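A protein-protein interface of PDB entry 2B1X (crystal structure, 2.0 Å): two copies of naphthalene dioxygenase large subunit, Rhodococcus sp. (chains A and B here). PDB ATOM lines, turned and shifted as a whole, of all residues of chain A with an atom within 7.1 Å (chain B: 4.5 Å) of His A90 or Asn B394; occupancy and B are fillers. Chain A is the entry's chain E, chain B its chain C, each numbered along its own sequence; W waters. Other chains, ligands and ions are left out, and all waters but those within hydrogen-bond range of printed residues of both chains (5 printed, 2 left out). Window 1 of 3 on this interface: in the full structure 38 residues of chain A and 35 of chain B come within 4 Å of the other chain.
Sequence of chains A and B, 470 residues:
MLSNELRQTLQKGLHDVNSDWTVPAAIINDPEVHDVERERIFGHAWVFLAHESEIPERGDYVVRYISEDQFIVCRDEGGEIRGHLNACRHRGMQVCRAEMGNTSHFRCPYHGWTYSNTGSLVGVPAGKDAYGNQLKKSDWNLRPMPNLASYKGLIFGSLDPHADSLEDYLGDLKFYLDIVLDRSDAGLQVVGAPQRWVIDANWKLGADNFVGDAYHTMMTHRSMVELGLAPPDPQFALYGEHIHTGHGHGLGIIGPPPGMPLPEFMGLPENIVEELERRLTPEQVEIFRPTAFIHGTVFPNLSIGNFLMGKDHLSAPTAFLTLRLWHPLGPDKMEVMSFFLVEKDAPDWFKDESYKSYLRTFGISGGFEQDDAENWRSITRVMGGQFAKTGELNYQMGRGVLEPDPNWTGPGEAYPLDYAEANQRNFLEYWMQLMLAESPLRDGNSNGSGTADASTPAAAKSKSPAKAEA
Hydrophobic or aromatic side chains of chain B that line the printed part of chain A: Tyr B215, Leu B393 and Tyr B395.
Of the 18 printed residues of chain A, 8 touch a printed residue of chain B.
Hydrophobic or aromatic side chains of chain A that line the printed part of chain B: His A90, His A111, Trp A113, Tyr A131, Leu A135 and Trp A140.
OH of Tyr B215 lies within hydrogen-bond range of NE1 of Trp A113, at 3.3 Å.
The guanidinium group (NH2) of Arg A89 is in salt-bridge range of the side-chain carboxylate (OE1) of Glu B392.
N of Asn B394 sits at hydrogen-bond distance from O of His A90 (3.0 Å).
NH1 of Arg A91 lies within hydrogen-bond range of O of Asn B394.
The side-chain amide nitrogen (ND2) of Asn B394 lies close to the indole nitrogen (NE1) of Trp A140, at 3.5 Å.
NE of Arg A91 lies close to OH of Tyr B395 (3.4 Å).
The indole nitrogen of Trp A140 sits at hydrogen-bond distance from the side-chain amide oxygen of Gln B396 (3.4 Å).
NE2 of His A90 sits at hydrogen-bond distance from OE2 of Glu B421 (2.7 Å).
OE2 of Glu B421 lies within salt-bridge range of NH2 of Arg A91, 3.0 Å away.
Water W3 lies within hydrogen-bond range of the side-chain hydroxyl (OH) of Tyr A131, the side-chain carboxylate (OE1) of Glu B421, the side-chain amide oxygen (OD1) of Asn B394 and a ring nitrogen (NE2) of His A90.
Water W1 lies within hydrogen-bond range of the backbone carbonyl oxygen (O) of Tyr B215 (2.7 Å) and the backbone carbonyl oxygen (O) of His A111 (3.0 Å).
Water W4 bridges the backbone carbonyl oxygen of Tyr A131 (2.7 Å) and the backbone carbonyl oxygen of Gln B396 (3.4 Å).
Water W5 lies within hydrogen-bond range of N of Lys A136 (2.7 Å) and OE1 of Gln B396 (3.4 Å).
Water W2 bridges the backbone carbonyl oxygen of Cys A88 (2.9 Å) and the backbone carbonyl oxygen of Glu B392 (3.3 Å).
The backbone carbonyl oxygen (O) of Trp B21 lies within hydrogen-bond range of the backbone NH (N) of Tyr B395, at 3.0 Å.
O of Trp B21 lies within hydrogen-bond range of N of Gln B396 (3.5 Å).
The backbone NH (N) of Gln B396 is in hydrogen-bond range of the side-chain amide oxygen (OD1) of Asn B394, at 3.0 Å.
The side-chain sulfur (SG) of Cys A88 lies close to the backbone NH (N) of His A90, at 3.5 Å.
The backbone NH (N) of Arg A89 is in hydrogen-bond range of the side-chain hydroxyl (OH) of Tyr A115 (3.0 Å).
The backbone NH (N) of Cys A108 sits at hydrogen-bond distance from the backbone carbonyl oxygen (O) of Trp A113 (3.0 Å).
No position is printed for both chains.
Of the 17 pairs that touch across the chains among the printed residues, none has its exchanged pair printed and touching as well.
His A90 touches just these residues of chain B: Leu B393 (3.6 Å), Asn B394 (3.0 Å) and Glu B421 (2.7 Å).
Printed residues of chain B within 4 Å of Tyr A131: Tyr B215 (3.6 Å).
Of the printed residues of chain A, Gln B396 touches Leu A135 (3.4 Å) and Trp A140 (3.4 Å).
Printed residues of chain B within 4 Å of Arg A91: Asn B394, Tyr B395 and Glu B421.
The nearest residue of chain A that does not touch Asn B394 is Tyr A131 (4.6 Å).
The nearest printed residue of chain B that does not touch Trp A140 is Leu B393 (5.4 Å).
Among the printed residues, pairs that only touch across the chains: Arg A89 with Asn B394, His A90 with Leu B393, His A111 with Tyr B215, Trp A113 with Asn B394, Tyr A131 with Tyr B215, Leu A135 with Asn B394, Leu A135 with Gln B396 and Trp A140 with Glu B392.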
ATOM      1  N   ALA A  87       2.591  26.732 -25.038  1.00  0.00           N
ATOM      2  CA  ALA A  87       1.535  26.226 -25.967  1.00  0.00           C
ATOM      3  C   ALA A  87       1.801  24.744 -26.156  1.00  0.00           C
ATOM      4  O   ALA A  87       2.838  24.369 -26.729  1.00  0.00           O
ATOM      5  CB  ALA A  87       1.619  26.951 -27.328  1.00  0.00           C
ATOM      6  N   CYS A  88       0.911  23.909 -25.624  1.00  0.00           N
ATOM      7  CA  CYS A  88       1.062  22.454 -25.735  1.00  0.00           C
ATOM      8  C   CYS A  88       1.240  22.037 -27.183  1.00  0.00           C
ATOM      9  O   CYS A  88       0.577  22.557 -28.087  1.00  0.00           O
ATOM     10  CB  CYS A  88      -0.172  21.770 -25.155  1.00  0.00           C
ATOM     11  SG  CYS A  88      -0.137  19.978 -25.075  1.00  0.00           S
ATOM     12  N   ARG A  89       2.085  21.041 -27.416  1.00  0.00           N
ATOM     13  CA  ARG A  89       2.342  20.603 -28.771  1.00  0.00           C
ATOM     14  C   ARG A  89       1.158  19.873 -29.364  1.00  0.00           C
ATOM     15  O   ARG A  89       1.108  19.678 -30.572  1.00  0.00           O
ATOM     16  CB  ARG A  89       3.595  19.708 -28.806  1.00  0.00           C
ATOM     17  CG  ARG A  89       4.870  20.430 -28.368  1.00  0.00           C
ATOM     18  CD  ARG A  89       5.200  21.706 -29.183  1.00  0.00           C
ATOM     19  NE  ARG A  89       5.282  21.426 -30.615  1.00  0.00           N
ATOM     20  CZ  ARG A  89       6.365  20.911 -31.224  1.00  0.00           C
ATOM     21  NH1 ARG A  89       7.488  20.629 -30.547  1.00  0.00           N
ATOM     22  NH2 ARG A  89       6.338  20.699 -32.519  1.00  0.00           N
ATOM     23  N   HIS A  90       0.221  19.459 -28.521  1.00  0.00           N
ATOM     24  CA  HIS A  90      -0.980  18.732 -29.007  1.00  0.00           C
ATOM     25  C   HIS A  90      -2.026  19.620 -29.722  1.00  0.00           C
ATOM     26  O   HIS A  90      -2.151  19.610 -30.943  1.00  0.00           O
ATOM     27  CB  HIS A  90      -1.581  17.904 -27.845  1.00  0.00           C
ATOM     28  CG  HIS A  90      -2.682  16.979 -28.244  1.00  0.00           C
ATOM     29  ND1 HIS A  90      -3.845  16.868 -27.512  1.00  0.00           N
ATOM     30  CD2 HIS A  90      -2.818  16.142 -29.307  1.00  0.00           C
ATOM     31  CE1 HIS A  90      -4.642  15.987 -28.097  1.00  0.00           C
ATOM     32  NE2 HIS A  90      -4.039  15.531 -29.180  1.00  0.00           N
ATOM     33  N   ARG A  91      -2.756  20.412 -28.957  1.00  0.00           N
ATOM     34  CA  ARG A  91      -3.723  21.345 -29.500  1.00  0.00           C
ATOM     35  C   ARG A  91      -3.455  22.780 -29.016  1.00  0.00           C
ATOM     36  O   ARG A  91      -4.298  23.634 -29.154  1.00  0.00           O
ATOM     37  CB  ARG A  91      -5.138  20.890 -29.127  1.00  0.00           C
ATOM     38  CG  ARG A  91      -6.253  21.384 -30.081  1.00  0.00           C
ATOM     39  CD  ARG A  91      -6.329  20.610 -31.384  1.00  0.00           C
ATOM     40  NE  ARG A  91      -6.902  19.276 -31.170  1.00  0.00           N
ATOM     41  CZ  ARG A  91      -6.205  18.121 -31.284  1.00  0.00           C
ATOM     42  NH1 ARG A  91      -4.915  18.143 -31.639  1.00  0.00           N
ATOM     43  NH2 ARG A  91      -6.815  16.950 -31.098  1.00  0.00           N
ATOM     44  N   GLY A  92      -2.285  23.042 -28.430  1.00  0.00           N
ATOM     45  CA  GLY A  92      -1.880  24.426 -28.196  1.00  0.00           C
ATOM     46  C   GLY A  92      -2.329  25.070 -26.898  1.00  0.00           C
ATOM     47  O   GLY A  92      -2.160  26.285 -26.738  1.00  0.00           O
ATOM     48  N   MET A  93      -2.876  24.298 -25.963  1.00  0.00           N
ATOM     49  CA  MET A  93      -3.247  24.893 -24.688  1.00  0.00           C
ATOM     50  C   MET A  93      -2.056  25.418 -23.897  1.00  0.00           C
ATOM     51  O   MET A  93      -0.930  24.884 -24.019  1.00  0.00           O
ATOM     52  CB  MET A  93      -4.076  23.941 -23.815  1.00  0.00           C
ATOM     53  CG  MET A  93      -4.970  24.829 -22.858  1.00  0.00           C
ATOM     54  SD  MET A  93      -5.855  23.909 -21.761  1.00  0.00           S
ATOM     55  CE  MET A  93      -6.007  25.135 -20.400  1.00  0.00           C
ATOM     56  N   CYS A 108      -0.662  19.558 -19.181  1.00  0.00           N
ATOM     57  CA  CYS A 108      -1.677  20.279 -19.948  1.00  0.00           C
ATOM     58  C   CYS A 108      -3.061  19.838 -19.464  1.00  0.00           C
ATOM     59  O   CYS A 108      -3.365  18.659 -19.483  1.00  0.00           O
ATOM     60  CB  CYS A 108      -1.501  19.997 -21.445  1.00  0.00           C
ATOM     61  SG  CYS A 108      -2.708  20.838 -22.431  1.00  0.00           S
ATOM     62  N   TYR A 110      -5.824  19.958 -20.970  1.00  0.00           N
ATOM     63  CA  TYR A 110      -6.778  19.533 -22.014  1.00  0.00           C
ATOM     64  C   TYR A 110      -6.761  17.982 -22.146  1.00  0.00           C
ATOM     65  O   TYR A 110      -7.773  17.326 -21.876  1.00  0.00           O
ATOM     66  CB  TYR A 110      -6.520  20.255 -23.344  1.00  0.00           C
ATOM     67  CG  TYR A 110      -7.649  20.249 -24.358  1.00  0.00           C
ATOM     68  CD1 TYR A 110      -7.534  20.968 -25.556  1.00  0.00           C
ATOM     69  CD2 TYR A 110      -8.830  19.500 -24.168  1.00  0.00           C
ATOM     70  CE1 TYR A 110      -8.558  20.962 -26.509  1.00  0.00           C
ATOM     71  CE2 TYR A 110      -9.843  19.499 -25.147  1.00  0.00           C
ATOM     72  CZ  TYR A 110      -9.703  20.248 -26.294  1.00  0.00           C
ATOM     73  OH  TYR A 110     -10.698  20.255 -27.245  1.00  0.00           O
ATOM     74  N   HIS A 111      -5.602  17.388 -22.494  1.00  0.00           N
ATOM     75  CA  HIS A 111      -5.546  15.917 -22.520  1.00  0.00           C
ATOM     76  C   HIS A 111      -4.491  15.287 -21.583  1.00  0.00           C
ATOM     77  O   HIS A 111      -4.291  14.062 -21.588  1.00  0.00           O
ATOM     78  CB  HIS A 111      -5.430  15.364 -23.942  1.00  0.00           C
ATOM     79  CG  HIS A 111      -6.339  16.031 -24.939  1.00  0.00           C
ATOM     80  ND1 HIS A 111      -6.085  17.291 -25.446  1.00  0.00           N
ATOM     81  CD2 HIS A 111      -7.480  15.603 -25.539  1.00  0.00           C
ATOM     82  CE1 HIS A 111      -7.022  17.597 -26.331  1.00  0.00           C
ATOM     83  NE2 HIS A 111      -7.876  16.586 -26.410  1.00  0.00           N
ATOM     84  N   GLY A 112      -3.817  16.126 -20.781  1.00  0.00           N
ATOM     85  CA  GLY A 112      -2.863  15.623 -19.812  1.00  0.00           C
ATOM     86  C   GLY A 112      -1.448  15.283 -20.270  1.00  0.00           C
ATOM     87  O   GLY A 112      -0.688  14.670 -19.502  1.00  0.00           O
ATOM     88  N   TRP A 113      -1.043  15.737 -21.453  1.00  0.00           N
ATOM     89  CA  TRP A 113       0.362  15.568 -21.884  1.00  0.00           C
ATOM     90  C   TRP A 113       1.196  16.259 -20.821  1.00  0.00           C
ATOM     91  O   TRP A 113       0.871  17.334 -20.384  1.00  0.00           O
ATOM     92  CB  TRP A 113       0.647  16.189 -23.257  1.00  0.00           C
ATOM     93  CG  TRP A 113       0.157  15.369 -24.443  1.00  0.00           C
ATOM     94  CD1 TRP A 113      -0.851  14.448 -24.449  1.00  0.00           C
ATOM     95  CD2 TRP A 113       0.613  15.474 -25.805  1.00  0.00           C
ATOM     96  NE1 TRP A 113      -1.047  13.963 -25.729  1.00  0.00           N
ATOM     97  CE2 TRP A 113      -0.152  14.563 -26.579  1.00  0.00           C
ATOM     98  CE3 TRP A 113       1.603  16.231 -26.451  1.00  0.00           C
ATOM     99  CZ2 TRP A 113       0.055  14.369 -27.961  1.00  0.00           C
ATOM    100  CZ3 TRP A 113       1.801  16.037 -27.835  1.00  0.00           C
ATOM    101  CH2 TRP A 113       1.009  15.130 -28.572  1.00  0.00           C
ATOM    102  N   TYR A 115       4.918  17.509 -19.370  1.00  0.00           N
ATOM    103  CA  TYR A 115       6.256  17.937 -19.741  1.00  0.00           C
ATOM    104  C   TYR A 115       7.138  18.192 -18.498  1.00  0.00           C
ATOM    105  O   TYR A 115       6.712  18.823 -17.525  1.00  0.00           O
ATOM    106  CB  TYR A 115       6.164  19.265 -20.532  1.00  0.00           C
ATOM    107  CG  TYR A 115       5.271  19.214 -21.793  1.00  0.00           C
ATOM    108  CD1 TYR A 115       3.894  19.489 -21.723  1.00  0.00           C
ATOM    109  CD2 TYR A 115       5.818  18.939 -23.041  1.00  0.00           C
ATOM    110  CE1 TYR A 115       3.112  19.468 -22.855  1.00  0.00           C
ATOM    111  CE2 TYR A 115       5.048  18.934 -24.188  1.00  0.00           C
ATOM    112  CZ  TYR A 115       3.695  19.184 -24.096  1.00  0.00           C
ATOM    113  OH  TYR A 115       2.936  19.147 -25.224  1.00  0.00           O
ATOM    114  N   TYR A 131      -2.359   5.704 -28.888  1.00  0.00           N
ATOM    115  CA  TYR A 131      -1.268   5.936 -29.838  1.00  0.00           C
ATOM    116  C   TYR A 131      -0.501   4.709 -30.282  1.00  0.00           C
ATOM    117  O   TYR A 131       0.350   4.812 -31.159  1.00  0.00           O
ATOM    118  CB  TYR A 131      -0.297   6.979 -29.275  1.00  0.00           C
ATOM    119  CG  TYR A 131      -0.876   8.365 -29.182  1.00  0.00           C
ATOM    120  CD1 TYR A 131      -1.515   8.770 -28.009  1.00  0.00           C
ATOM    121  CD2 TYR A 131      -0.756   9.296 -30.241  1.00  0.00           C
ATOM    122  CE1 TYR A 131      -2.041  10.056 -27.864  1.00  0.00           C
ATOM    123  CE2 TYR A 131      -1.294  10.593 -30.111  1.00  0.00           C
ATOM    124  CZ  TYR A 131      -1.923  10.960 -28.895  1.00  0.00           C
ATOM    125  OH  TYR A 131      -2.471  12.190 -28.651  1.00  0.00           O
ATOM    126  N   LEU A 135       3.753   7.334 -31.001  1.00  0.00           N
ATOM    127  CA  LEU A 135       4.097   8.746 -30.842  1.00  0.00           C
ATOM    128  C   LEU A 135       5.500   8.904 -30.267  1.00  0.00           C
ATOM    129  O   LEU A 135       5.755   8.455 -29.148  1.00  0.00           O
ATOM    130  CB  LEU A 135       3.082   9.471 -29.965  1.00  0.00           C
ATOM    131  CG  LEU A 135       3.337  10.979 -29.772  1.00  0.00           C
ATOM    132  CD1 LEU A 135       2.794  11.800 -30.948  1.00  0.00           C
ATOM    133  CD2 LEU A 135       2.699  11.442 -28.472  1.00  0.00           C
ATOM    134  N   LYS A 136       6.388   9.525 -31.049  1.00  0.00           N
ATOM    135  CA  LYS A 136       7.765   9.779 -30.651  1.00  0.00           C
ATOM    136  C   LYS A 136       7.785  11.046 -29.808  1.00  0.00           C
ATOM    137  O   LYS A 136       7.831  12.169 -30.352  1.00  0.00           O
ATOM    138  CB  LYS A 136       8.667   9.928 -31.877  1.00  0.00           C
ATOM    139  CG  LYS A 136      10.175  10.044 -31.561  1.00  0.00           C
ATOM    140  CD  LYS A 136      10.998   9.864 -32.822  1.00  0.00           C
ATOM    141  CE  LYS A 136      12.370  10.494 -32.665  1.00  0.00           C
ATOM    142  NZ  LYS A 136      13.282   9.545 -31.974  1.00  0.00           N
ATOM    143  N   ASP A 139       9.941  14.202 -30.285  1.00  0.00           N
ATOM    144  CA  ASP A 139       9.647  15.098 -31.407  1.00  0.00           C
ATOM    145  C   ASP A 139       8.669  16.201 -30.989  1.00  0.00           C
ATOM    146  O   ASP A 139       8.449  17.139 -31.747  1.00  0.00           O
ATOM    147  CB  ASP A 139       9.044  14.313 -32.578  1.00  0.00           C
ATOM    148  CG  ASP A 139      10.107  13.607 -33.416  1.00  0.00           C
ATOM    149  OD1 ASP A 139       9.745  12.883 -34.367  1.00  0.00           O
ATOM    150  OD2 ASP A 139      11.322  13.723 -33.177  1.00  0.00           O
ATOM    151  N   TRP A 140       8.092  16.075 -29.789  1.00  0.00           N
ATOM    152  CA  TRP A 140       6.989  16.955 -29.330  1.00  0.00           C
ATOM    153  C   TRP A 140       7.282  17.569 -27.960  1.00  0.00           C
ATOM    154  O   TRP A 140       6.401  17.793 -27.123  1.00  0.00           O
ATOM    155  CB  TRP A 140       5.641  16.212 -29.388  1.00  0.00           C
ATOM    156  CG  TRP A 140       5.431  15.634 -30.784  1.00  0.00           C
ATOM    157  CD1 TRP A 140       5.719  14.368 -31.188  1.00  0.00           C
ATOM    158  CD2 TRP A 140       5.006  16.340 -31.960  1.00  0.00           C
ATOM    159  NE1 TRP A 140       5.470  14.231 -32.529  1.00  0.00           N
ATOM    160  CE2 TRP A 140       5.035  15.418 -33.037  1.00  0.00           C
ATOM    161  CE3 TRP A 140       4.580  17.649 -32.215  1.00  0.00           C
ATOM    162  CZ2 TRP A 140       4.637  15.754 -34.338  1.00  0.00           C
ATOM    163  CZ3 TRP A 140       4.183  17.971 -33.522  1.00  0.00           C
ATOM    164  CH2 TRP A 140       4.247  17.039 -34.558  1.00  0.00           C
ATOM    165  N   TRP B  21       0.032  13.644 -40.416  1.00  0.00           N
ATOM    166  CA  TRP B  21      -1.158  13.755 -39.547  1.00  0.00           C
ATOM    167  C   TRP B  21      -1.031  14.982 -38.620  1.00  0.00           C
ATOM    168  O   TRP B  21      -1.266  14.896 -37.414  1.00  0.00           O
ATOM    169  CB  TRP B  21      -1.439  12.469 -38.749  1.00  0.00           C
ATOM    170  CG  TRP B  21      -1.813  11.230 -39.591  1.00  0.00           C
ATOM    171  CD1 TRP B  21      -1.484  10.983 -40.898  1.00  0.00           C
ATOM    172  CD2 TRP B  21      -2.606  10.111 -39.166  1.00  0.00           C
ATOM    173  NE1 TRP B  21      -2.016   9.777 -41.307  1.00  0.00           N
ATOM    174  CE2 TRP B  21      -2.706   9.218 -40.267  1.00  0.00           C
ATOM    175  CE3 TRP B  21      -3.248   9.771 -37.960  1.00  0.00           C
ATOM    176  CZ2 TRP B  21      -3.409   8.005 -40.204  1.00  0.00           C
ATOM    177  CZ3 TRP B  21      -3.941   8.549 -37.893  1.00  0.00           C
ATOM    178  CH2 TRP B  21      -4.013   7.685 -39.014  1.00  0.00           C
ATOM    179  N   TYR B 215     -10.804  11.434 -25.834  1.00  0.00           N
ATOM    180  CA  TYR B 215      -9.501  11.475 -25.138  1.00  0.00           C
ATOM    181  C   TYR B 215      -9.432  12.530 -24.013  1.00  0.00           C
ATOM    182  O   TYR B 215      -8.925  12.254 -22.906  1.00  0.00           O
ATOM    183  CB  TYR B 215      -8.398  11.695 -26.197  1.00  0.00           C
ATOM    184  CG  TYR B 215      -6.953  11.654 -25.749  1.00  0.00           C
ATOM    185  CD1 TYR B 215      -6.494  10.684 -24.865  1.00  0.00           C
ATOM    186  CD2 TYR B 215      -6.025  12.591 -26.258  1.00  0.00           C
ATOM    187  CE1 TYR B 215      -5.162  10.642 -24.467  1.00  0.00           C
ATOM    188  CE2 TYR B 215      -4.677  12.557 -25.870  1.00  0.00           C
ATOM    189  CZ  TYR B 215      -4.259  11.601 -24.963  1.00  0.00           C
ATOM    190  OH  TYR B 215      -2.929  11.548 -24.599  1.00  0.00           O
ATOM    191  N   GLU B 392       2.664  23.436 -35.544  1.00  0.00           N
ATOM    192  CA  GLU B 392       1.661  22.518 -36.049  1.00  0.00           C
ATOM    193  C   GLU B 392       0.843  21.992 -34.887  1.00  0.00           C
ATOM    194  O   GLU B 392       1.266  22.044 -33.723  1.00  0.00           O
ATOM    195  CB  GLU B 392       2.343  21.376 -36.836  1.00  0.00           C
ATOM    196  CG  GLU B 392       3.190  20.452 -35.974  1.00  0.00           C
ATOM    197  CD  GLU B 392       4.611  20.962 -35.706  1.00  0.00           C
ATOM    198  OE1 GLU B 392       4.804  21.793 -34.790  1.00  0.00           O
ATOM    199  OE2 GLU B 392       5.557  20.506 -36.392  1.00  0.00           O
ATOM    200  N   LEU B 393      -0.349  21.518 -35.196  1.00  0.00           N
ATOM    201  CA  LEU B 393      -1.176  20.814 -34.220  1.00  0.00           C
ATOM    202  C   LEU B 393      -0.998  19.329 -34.483  1.00  0.00           C
ATOM    203  O   LEU B 393      -1.017  18.913 -35.640  1.00  0.00           O
ATOM    204  CB  LEU B 393      -2.649  21.214 -34.379  1.00  0.00           C
ATOM    205  CG  LEU B 393      -3.008  22.721 -34.349  1.00  0.00           C
ATOM    206  CD1 LEU B 393      -4.440  22.948 -34.814  1.00  0.00           C
ATOM    207  CD2 LEU B 393      -2.800  23.321 -32.960  1.00  0.00           C
ATOM    208  N   ASN B 394      -0.873  18.542 -33.420  1.00  0.00           N
ATOM    209  CA  ASN B 394      -0.608  17.122 -33.540  1.00  0.00           C
ATOM    210  C   ASN B 394      -1.932  16.359 -33.598  1.00  0.00           C
ATOM    211  O   ASN B 394      -2.669  16.319 -32.614  1.00  0.00           O
ATOM    212  CB  ASN B 394       0.306  16.640 -32.380  1.00  0.00           C
ATOM    213  CG  ASN B 394       0.763  15.194 -32.530  1.00  0.00           C
ATOM    214  OD1 ASN B 394      -0.044  14.264 -32.541  1.00  0.00           O
ATOM    215  ND2 ASN B 394       2.097  14.995 -32.574  1.00  0.00           N
ATOM    216  N   TYR B 395      -2.228  15.785 -34.766  1.00  0.00           N
ATOM    217  CA  TYR B 395      -3.371  14.877 -34.917  1.00  0.00           C
ATOM    218  C   TYR B 395      -2.974  13.439 -35.206  1.00  0.00           C
ATOM    219  O   TYR B 395      -3.661  12.717 -35.962  1.00  0.00           O
ATOM    220  CB  TYR B 395      -4.298  15.405 -36.001  1.00  0.00           C
ATOM    221  CG  TYR B 395      -5.059  16.627 -35.577  1.00  0.00           C
ATOM    222  CD1 TYR B 395      -4.652  17.899 -35.979  1.00  0.00           C
ATOM    223  CD2 TYR B 395      -6.197  16.514 -34.779  1.00  0.00           C
ATOM    224  CE1 TYR B 395      -5.382  19.036 -35.613  1.00  0.00           C
ATOM    225  CE2 TYR B 395      -6.936  17.632 -34.424  1.00  0.00           C
ATOM    226  CZ  TYR B 395      -6.519  18.900 -34.838  1.00  0.00           C
ATOM    227  OH  TYR B 395      -7.263  20.035 -34.496  1.00  0.00           O
ATOM    228  N   GLN B 396      -1.886  13.020 -34.568  1.00  0.00           N
ATOM    229  CA  GLN B 396      -1.221  11.762 -34.886  1.00  0.00           C
ATOM    230  C   GLN B 396      -1.792  10.534 -34.168  1.00  0.00           C
ATOM    231  O   GLN B 396      -1.284   9.445 -34.327  1.00  0.00           O
ATOM    232  CB  GLN B 396       0.274  11.885 -34.602  1.00  0.00           C
ATOM    233  CG  GLN B 396       0.996  12.932 -35.488  1.00  0.00           C
ATOM    234  CD  GLN B 396       2.514  12.832 -35.376  1.00  0.00           C
ATOM    235  OE1 GLN B 396       3.031  12.638 -34.272  1.00  0.00           O
ATOM    236  NE2 GLN B 396       3.210  12.958 -36.488  1.00  0.00           N
ATOM    237  N   GLU B 421      -7.942  10.334 -33.923  1.00  0.00           N
ATOM    238  CA  GLU B 421      -8.088  11.709 -34.430  1.00  0.00           C
ATOM    239  C   GLU B 421      -8.410  11.753 -35.944  1.00  0.00           C
ATOM    240  O   GLU B 421      -8.241  12.787 -36.610  1.00  0.00           O
ATOM    241  CB  GLU B 421      -6.835  12.521 -34.054  1.00  0.00           C
ATOM    242  CG  GLU B 421      -6.882  13.008 -32.595  1.00  0.00           C
ATOM    243  CD  GLU B 421      -5.561  13.503 -31.986  1.00  0.00           C
ATOM    244  OE1 GLU B 421      -4.453  13.236 -32.510  1.00  0.00           O
ATOM    245  OE2 GLU B 421      -5.640  14.179 -30.921  1.00  0.00           O
HETATM  246  O   HOH W   1      -7.069  13.004 -21.152  1.00  0.00           O
HETATM  247  O   HOH W   2       0.216  23.318 -30.902  1.00  0.00           O
HETATM  248  O   HOH W   3      -2.243  13.430 -30.967  1.00  0.00           O
HETATM  249  O   HOH W   4      -0.532   6.335 -33.197  1.00  0.00           O
HETATM  250  O   HOH W   5       5.608  10.685 -33.373  1.00  0.00           O
